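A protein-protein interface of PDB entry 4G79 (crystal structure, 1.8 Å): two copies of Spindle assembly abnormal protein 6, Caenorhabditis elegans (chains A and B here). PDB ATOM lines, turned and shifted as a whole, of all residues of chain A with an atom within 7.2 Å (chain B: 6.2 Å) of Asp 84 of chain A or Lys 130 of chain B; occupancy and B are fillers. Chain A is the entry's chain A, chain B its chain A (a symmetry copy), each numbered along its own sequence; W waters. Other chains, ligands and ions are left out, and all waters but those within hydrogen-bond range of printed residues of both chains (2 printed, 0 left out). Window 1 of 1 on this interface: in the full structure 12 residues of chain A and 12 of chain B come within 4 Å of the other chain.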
ATOM      1  N   ILE A  78     -10.629   2.287 -22.984  1.00  0.00           N
ATOM      2  CA  ILE A  78      -9.314   2.785 -23.412  1.00  0.00           C
ATOM      3  C   ILE A  78      -8.877   3.909 -22.444  1.00  0.00           C
ATOM      4  O   ILE A  78      -7.756   3.879 -21.920  1.00  0.00           O
ATOM      5  CB  ILE A  78      -9.326   3.261 -24.898  1.00  0.00           C
ATOM      6  CG1 ILE A  78      -9.471   2.051 -25.859  1.00  0.00           C
ATOM      7  CG2 ILE A  78      -8.059   4.068 -25.228  1.00  0.00           C
ATOM      8  CD1 ILE A  78      -9.784   2.403 -27.338  1.00  0.00           C
ATOM      9  N   LEU A  79      -9.791   4.859 -22.176  1.00  0.00           N
ATOM     10  CA  LEU A  79      -9.556   5.979 -21.266  1.00  0.00           C
ATOM     11  C   LEU A  79      -9.172   5.495 -19.866  1.00  0.00           C
ATOM     12  O   LEU A  79      -8.232   6.041 -19.279  1.00  0.00           O
ATOM     13  CB  LEU A  79     -10.797   6.893 -21.181  1.00  0.00           C
ATOM     14  CG  LEU A  79     -10.584   8.199 -20.391  1.00  0.00           C
ATOM     15  CD1 LEU A  79      -9.966   9.259 -21.258  1.00  0.00           C
ATOM     16  CD2 LEU A  79     -11.883   8.696 -19.753  1.00  0.00           C
ATOM     17  N   ALA A  80      -9.891   4.500 -19.329  1.00  0.00           N
ATOM     18  CA  ALA A  80      -9.648   3.966 -17.995  1.00  0.00           C
ATOM     19  C   ALA A  80      -8.257   3.303 -17.913  1.00  0.00           C
ATOM     20  O   ALA A  80      -7.536   3.488 -16.926  1.00  0.00           O
ATOM     21  CB  ALA A  80     -10.746   2.978 -17.622  1.00  0.00           C
ATOM     22  N   ARG A  81      -7.879   2.570 -18.981  1.00  0.00           N
ATOM     23  CA  ARG A  81      -6.585   1.904 -19.106  1.00  0.00           C
ATOM     24  C   ARG A  81      -5.466   2.954 -19.162  1.00  0.00           C
ATOM     25  O   ARG A  81      -4.502   2.856 -18.399  1.00  0.00           O
ATOM     26  CB  ARG A  81      -6.568   1.005 -20.358  1.00  0.00           C
ATOM     27  CG  ARG A  81      -5.352   0.079 -20.458  1.00  0.00           C
ATOM     28  CD  ARG A  81      -4.578   0.238 -21.766  1.00  0.00           C
ATOM     29  NE  ARG A  81      -5.355  -0.178 -22.938  1.00  0.00           N
ATOM     30  CZ  ARG A  81      -5.516   0.556 -24.036  1.00  0.00           C
ATOM     31  NH1 ARG A  81      -4.944   1.751 -24.136  1.00  0.00           N
ATOM     32  NH2 ARG A  81      -6.243   0.098 -25.046  1.00  0.00           N
ATOM     33  N   ASP A  82      -5.623   3.976 -20.018  1.00  0.00           N
ATOM     34  CA  ASP A  82      -4.635   5.046 -20.196  1.00  0.00           C
ATOM     35  C   ASP A  82      -4.416   5.892 -18.953  1.00  0.00           C
ATOM     36  O   ASP A  82      -3.293   6.341 -18.729  1.00  0.00           O
ATOM     37  CB  ASP A  82      -5.033   5.988 -21.350  1.00  0.00           C
ATOM     38  CG  ASP A  82      -5.025   5.398 -22.751  1.00  0.00           C
ATOM     39  OD1 ASP A  82      -4.619   4.225 -22.905  1.00  0.00           O
ATOM     40  OD2 ASP A  82      -5.432   6.110 -23.694  1.00  0.00           O
ATOM     41  N   HIS A  83      -5.469   6.125 -18.163  1.00  0.00           N
ATOM     42  CA  HIS A  83      -5.428   7.002 -16.998  1.00  0.00           C
ATOM     43  C   HIS A  83      -5.586   6.300 -15.654  1.00  0.00           C
ATOM     44  O   HIS A  83      -5.756   7.001 -14.659  1.00  0.00           O
ATOM     45  CB  HIS A  83      -6.510   8.097 -17.140  1.00  0.00           C
ATOM     46  CG  HIS A  83      -6.225   8.985 -18.288  1.00  0.00           C
ATOM     47  ND1 HIS A  83      -5.242   9.944 -18.209  1.00  0.00           N
ATOM     48  CD2 HIS A  83      -6.685   8.930 -19.556  1.00  0.00           C
ATOM     49  CE1 HIS A  83      -5.176  10.487 -19.413  1.00  0.00           C
ATOM     50  NE2 HIS A  83      -6.029   9.912 -20.255  1.00  0.00           N
ATOM     51  N   ASP A  84      -5.485   4.958 -15.589  1.00  0.00           N
ATOM     52  CA  ASP A  84      -5.568   4.175 -14.347  1.00  0.00           C
ATOM     53  C   ASP A  84      -6.871   4.400 -13.569  1.00  0.00           C
ATOM     54  O   ASP A  84      -6.871   4.335 -12.336  1.00  0.00           O
ATOM     55  CB  ASP A  84      -4.361   4.485 -13.424  1.00  0.00           C
ATOM     56  CG  ASP A  84      -3.094   3.714 -13.740  1.00  0.00           C
ATOM     57  OD1 ASP A  84      -3.143   2.818 -14.622  1.00  0.00           O
ATOM     58  OD2 ASP A  84      -2.050   4.013 -13.111  1.00  0.00           O
ATOM     59  N   LEU A  85      -7.990   4.599 -14.280  1.00  0.00           N
ATOM     60  CA  LEU A  85      -9.283   4.778 -13.630  1.00  0.00           C
ATOM     61  C   LEU A  85      -9.750   3.454 -13.076  1.00  0.00           C
ATOM     62  O   LEU A  85      -9.593   2.416 -13.733  1.00  0.00           O
ATOM     63  CB  LEU A  85     -10.321   5.379 -14.613  1.00  0.00           C
ATOM     64  CG  LEU A  85      -9.938   6.704 -15.286  1.00  0.00           C
ATOM     65  CD1 LEU A  85     -11.058   7.192 -16.231  1.00  0.00           C
ATOM     66  CD2 LEU A  85      -9.614   7.806 -14.236  1.00  0.00           C
ATOM     67  N   THR A  86     -10.304   3.462 -11.859  1.00  0.00           N
ATOM     68  CA  THR A  86     -10.730   2.194 -11.246  1.00  0.00           C
ATOM     69  C   THR A  86     -12.243   2.048 -11.192  1.00  0.00           C
ATOM     70  O   THR A  86     -12.737   1.055 -10.658  1.00  0.00           O
ATOM     71  CB  THR A  86     -10.129   2.035  -9.869  1.00  0.00           C
ATOM     72  OG1 THR A  86     -10.525   3.160  -9.078  1.00  0.00           O
ATOM     73  CG2 THR A  86      -8.618   1.899  -9.924  1.00  0.00           C
ATOM     74  N   VAL A  87     -12.979   3.016 -11.766  1.00  0.00           N
ATOM     75  CA  VAL A  87     -14.455   2.957 -11.799  1.00  0.00           C
ATOM     76  C   VAL A  87     -14.895   2.502 -13.187  1.00  0.00           C
ATOM     77  O   VAL A  87     -14.196   2.745 -14.163  1.00  0.00           O
ATOM     78  CB  VAL A  87     -15.146   4.304 -11.370  1.00  0.00           C
ATOM     79  CG1 VAL A  87     -14.845   4.615  -9.908  1.00  0.00           C
ATOM     80  CG2 VAL A  87     -14.732   5.478 -12.260  1.00  0.00           C
ATOM     81  N   ILE A 133      -6.394  13.165 -13.067  1.00  0.00           N
ATOM     82  CA  ILE A 133      -7.447  12.153 -13.029  1.00  0.00           C
ATOM     83  C   ILE A 133      -7.562  11.562 -14.435  1.00  0.00           C
ATOM     84  O   ILE A 133      -7.393  10.345 -14.623  1.00  0.00           O
ATOM     85  CB  ILE A 133      -8.773  12.752 -12.496  1.00  0.00           C
ATOM     86  CG1 ILE A 133      -8.543  13.358 -11.074  1.00  0.00           C
ATOM     87  CG2 ILE A 133      -9.866  11.655 -12.458  1.00  0.00           C
ATOM     88  CD1 ILE A 133      -9.768  14.085 -10.476  1.00  0.00           C
ATOM     89  N   GLU B 106      -0.417   1.979  -1.122  1.00  0.00           N
ATOM     90  CA  GLU B 106      -0.331   0.653  -1.734  1.00  0.00           C
ATOM     91  C   GLU B 106       0.954   0.554  -2.536  1.00  0.00           C
ATOM     92  O   GLU B 106       1.263   1.458  -3.318  1.00  0.00           O
ATOM     93  CB  GLU B 106      -1.541   0.353  -2.642  1.00  0.00           C
ATOM     94  CG  GLU B 106      -2.909   0.603  -2.021  1.00  0.00           C
ATOM     95  CD  GLU B 106      -3.437   1.997  -2.304  1.00  0.00           C
ATOM     96  OE1 GLU B 106      -3.633   2.323  -3.495  1.00  0.00           O
ATOM     97  OE2 GLU B 106      -3.602   2.782  -1.344  1.00  0.00           O
ATOM     98  N   ASN B 108       3.225  -1.816  -5.246  1.00  0.00           N
ATOM     99  CA  ASN B 108       3.346  -2.964  -6.158  1.00  0.00           C
ATOM    100  C   ASN B 108       4.787  -3.143  -6.499  1.00  0.00           C
ATOM    101  O   ASN B 108       5.478  -2.155  -6.788  1.00  0.00           O
ATOM    102  CB  ASN B 108       2.584  -2.823  -7.480  1.00  0.00           C
ATOM    103  CG  ASN B 108       1.096  -2.913  -7.424  1.00  0.00           C
ATOM    104  OD1 ASN B 108       0.503  -3.323  -6.430  1.00  0.00           O
ATOM    105  ND2 ASN B 108       0.466  -2.502  -8.514  1.00  0.00           N
ATOM    106  N   PHE B 123       1.528   3.984  -4.670  1.00  0.00           N
ATOM    107  CA  PHE B 123       0.214   4.535  -5.016  1.00  0.00           C
ATOM    108  C   PHE B 123      -0.442   5.126  -3.849  1.00  0.00           C
ATOM    109  O   PHE B 123      -0.131   4.750  -2.734  1.00  0.00           O
ATOM    110  CB  PHE B 123      -0.737   3.436  -5.556  1.00  0.00           C
ATOM    111  CG  PHE B 123      -0.282   2.720  -6.802  1.00  0.00           C
ATOM    112  CD1 PHE B 123       0.622   1.658  -6.724  1.00  0.00           C
ATOM    113  CD2 PHE B 123      -0.802   3.057  -8.047  1.00  0.00           C
ATOM    114  CE1 PHE B 123       1.014   0.970  -7.872  1.00  0.00           C
ATOM    115  CE2 PHE B 123      -0.396   2.379  -9.200  1.00  0.00           C
ATOM    116  CZ  PHE B 123       0.496   1.329  -9.100  1.00  0.00           C
ATOM    117  N   SER B 124      -1.390   6.024  -4.094  1.00  0.00           N
ATOM    118  CA  SER B 124      -2.279   6.556  -3.063  1.00  0.00           C
ATOM    119  C   SER B 124      -3.677   6.632  -3.715  1.00  0.00           C
ATOM    120  O   SER B 124      -3.995   7.611  -4.392  1.00  0.00           O
ATOM    121  CB  SER B 124      -1.770   7.891  -2.535  1.00  0.00           C
ATOM    122  OG  SER B 124      -2.585   8.321  -1.460  1.00  0.00           O
ATOM    123  N   LYS B 125      -4.453   5.535  -3.621  1.00  0.00           N
ATOM    124  CA  LYS B 125      -5.752   5.403  -4.297  1.00  0.00           C
ATOM    125  C   LYS B 125      -6.714   6.488  -3.923  1.00  0.00           C
ATOM    126  O   LYS B 125      -6.663   7.060  -2.841  1.00  0.00           O
ATOM    127  CB  LYS B 125      -6.421   4.018  -4.070  1.00  0.00           C
ATOM    128  CG  LYS B 125      -6.910   3.738  -2.654  1.00  0.00           C
ATOM    129  CD  LYS B 125      -7.888   2.546  -2.610  1.00  0.00           C
ATOM    130  CE  LYS B 125      -8.371   2.259  -1.205  1.00  0.00           C
ATOM    131  NZ  LYS B 125      -9.243   3.341  -0.659  1.00  0.00           N
ATOM    132  N   THR B 126      -7.512   6.854  -4.907  1.00  0.00           N
ATOM    133  CA  THR B 126      -8.594   7.809  -4.771  1.00  0.00           C
ATOM    134  C   THR B 126      -9.882   7.042  -5.116  1.00  0.00           C
ATOM    135  O   THR B 126      -9.807   5.911  -5.624  1.00  0.00           O
ATOM    136  CB  THR B 126      -8.362   9.037  -5.695  1.00  0.00           C
ATOM    137  OG1 THR B 126      -8.857   8.713  -6.996  1.00  0.00           O
ATOM    138  CG2 THR B 126      -6.887   9.502  -5.757  1.00  0.00           C
ATOM    139  N   ILE B 128     -11.536   7.378  -7.712  1.00  0.00           N
ATOM    140  CA  ILE B 128     -11.639   7.311  -9.180  1.00  0.00           C
ATOM    141  C   ILE B 128     -10.476   6.607  -9.810  1.00  0.00           C
ATOM    142  O   ILE B 128     -10.612   6.103 -10.918  1.00  0.00           O
ATOM    143  CB  ILE B 128     -11.710   8.751  -9.804  1.00  0.00           C
ATOM    144  CG1 ILE B 128     -12.523   9.733  -8.930  1.00  0.00           C
ATOM    145  CG2 ILE B 128     -12.234   8.713 -11.272  1.00  0.00           C
ATOM    146  CD1 ILE B 128     -12.641  11.184  -9.420  1.00  0.00           C
ATOM    147  N   SER B 129      -9.324   6.645  -9.178  1.00  0.00           N
ATOM    148  CA  SER B 129      -8.149   6.107  -9.842  1.00  0.00           C
ATOM    149  C   SER B 129      -7.148   5.465  -8.896  1.00  0.00           C
ATOM    150  O   SER B 129      -7.231   5.612  -7.677  1.00  0.00           O
ATOM    151  CB  SER B 129      -7.441   7.218 -10.612  1.00  0.00           C
ATOM    152  OG  SER B 129      -6.789   8.088  -9.710  1.00  0.00           O
ATOM    153  N   LYS B 130      -6.172   4.781  -9.495  1.00  0.00           N
ATOM    154  CA  LYS B 130      -5.099   4.094  -8.748  1.00  0.00           C
ATOM    155  C   LYS B 130      -4.226   5.077  -7.972  1.00  0.00           C
ATOM    156  O   LYS B 130      -3.732   4.698  -6.918  1.00  0.00           O
ATOM    157  CB  LYS B 130      -4.237   3.254  -9.687  1.00  0.00           C
ATOM    158  CG  LYS B 130      -4.980   2.047 -10.223  1.00  0.00           C
ATOM    159  CD  LYS B 130      -4.107   1.235 -11.152  1.00  0.00           C
ATOM    160  CE  LYS B 130      -4.828   0.003 -11.635  1.00  0.00           C
ATOM    161  NZ  LYS B 130      -3.894  -0.960 -12.270  1.00  0.00           N
ATOM    162  N   GLY B 131      -4.105   6.335  -8.447  1.00  0.00           N
ATOM    163  CA  GLY B 131      -3.312   7.356  -7.775  1.00  0.00           C
ATOM    164  C   GLY B 131      -1.833   7.017  -7.670  1.00  0.00           C
ATOM    165  O   GLY B 131      -1.225   7.238  -6.619  1.00  0.00           O
ATOM    166  N   LYS B 132      -1.218   6.558  -8.772  1.00  0.00           N
ATOM    167  CA  LYS B 132       0.233   6.278  -8.762  1.00  0.00           C
ATOM    168  C   LYS B 132       1.032   7.523  -8.406  1.00  0.00           C
ATOM    169  O   LYS B 132       0.798   8.590  -8.981  1.00  0.00           O
ATOM    170  CB  LYS B 132       0.730   5.731 -10.109  1.00  0.00           C
ATOM    171  CG  LYS B 132       2.155   5.135 -10.013  1.00  0.00           C
ATOM    172  CD  LYS B 132       2.822   4.987 -11.367  1.00  0.00           C
ATOM    173  CE  LYS B 132       2.778   3.594 -11.932  1.00  0.00           C
ATOM    174  NZ  LYS B 132       3.551   3.496 -13.203  1.00  0.00           N
HETATM  175  O   HOH W   1      -9.306   3.434  -6.785  1.00  0.00           O
HETATM  176  O   HOH W   2      -2.277   6.237 -11.430  1.00  0.00           O
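The backbone carbonyl oxygen (O) of Asp 84 of chain A lies within hydrogen-bond range of the backbone NH (N) of Lys 130 of chain B, at 3.0 Å.
The backbone NH (N) of Thr 86 of chain A sits at hydrogen-bond distance from the backbone carbonyl oxygen (O) of Ile 128 of chain B (2.8 Å).
N of Leu 85 of chain A lies within hydrogen-bond range of O of Ala 80 of chain A, at 2.9 Å.
The backbone NH (N) of Lys 125 of chain B lies close to the backbone carbonyl oxygen (O) of Lys 130 of chain B, 3.5 Å away.
OG1 of Thr 126 of chain B is in hydrogen-bond range of N of Ile 128 of chain B, at 3.1 Å.
The side-chain hydroxyl (OG1) of Thr 126 of chain B lies within hydrogen-bond range of the backbone NH (N) of Ser 129 of chain B (3.0 Å).
OG of Ser 129 of chain B sits close to N of Gly 131 of chain B (3.4 Å).
Among the printed residues, pairs that only touch across the chains: Asp 84 of chain A with Ser 129 of chain B (3.3 Å), Leu 85 of chain A with Ile 128 of chain B (3.3 Å), Thr 86 of chain A with Ser 129 of chain B (3.7 Å), Thr 86 of chain A with Lys 130 of chain B (3.7 Å), Val 87 of chain A with Ile 128 of chain B (3.98 Å) and Ile 133 of chain A with Ile 128 of chain B (3.96 Å).
Asp 84 of chain A touches just these residues of chain B: Ser 129 (3.3 Å) and Lys 130 (3.0 Å).
Of the printed residues of chain B, Leu 85 of chain A touches Ile 128 (3.3 Å).
Printed residues of chain B within 4 Å of Ile 133 of chain A: Ile 128 (3.96 Å).
Lys 132 of chain B touches none of the printed residues of chain A.
The nearest printed residue of chain B that does not touch Val 87 of chain A is Ser 129 of chain B (5.8 Å).
Printed residues of chain A that touch a printed residue of chain B: Asp 84, Leu 85, Thr 86, Val 87 and Ile 133.
Hydrophobic or aromatic side chains of chain A that line the printed part of chain B: Leu 85 and Ile 133.
Among the printed residues, no Asp or Glu carboxylate lies within 4 Å of a Lys or Arg side-chain nitrogen of the other chain.
No position is printed for both chains.
Of the 8 pairs that touch across the chains among the printed residues, none has its exchanged pair printed and touching as well.
Water W1 lies within hydrogen-bond range of the side-chain hydroxyl of Thr 86 of chain A (2.6 Å), the backbone carbonyl oxygen of Thr 126 of chain B (2.8 Å) and the backbone carbonyl oxygen of Ser 129 of chain B (3.1 Å).
Water W2 lies within hydrogen-bond range of the side-chain carboxylate of Asp 84 of chain A, the backbone NH of Lys 132 of chain B and the backbone NH of Gly 131 of chain B.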
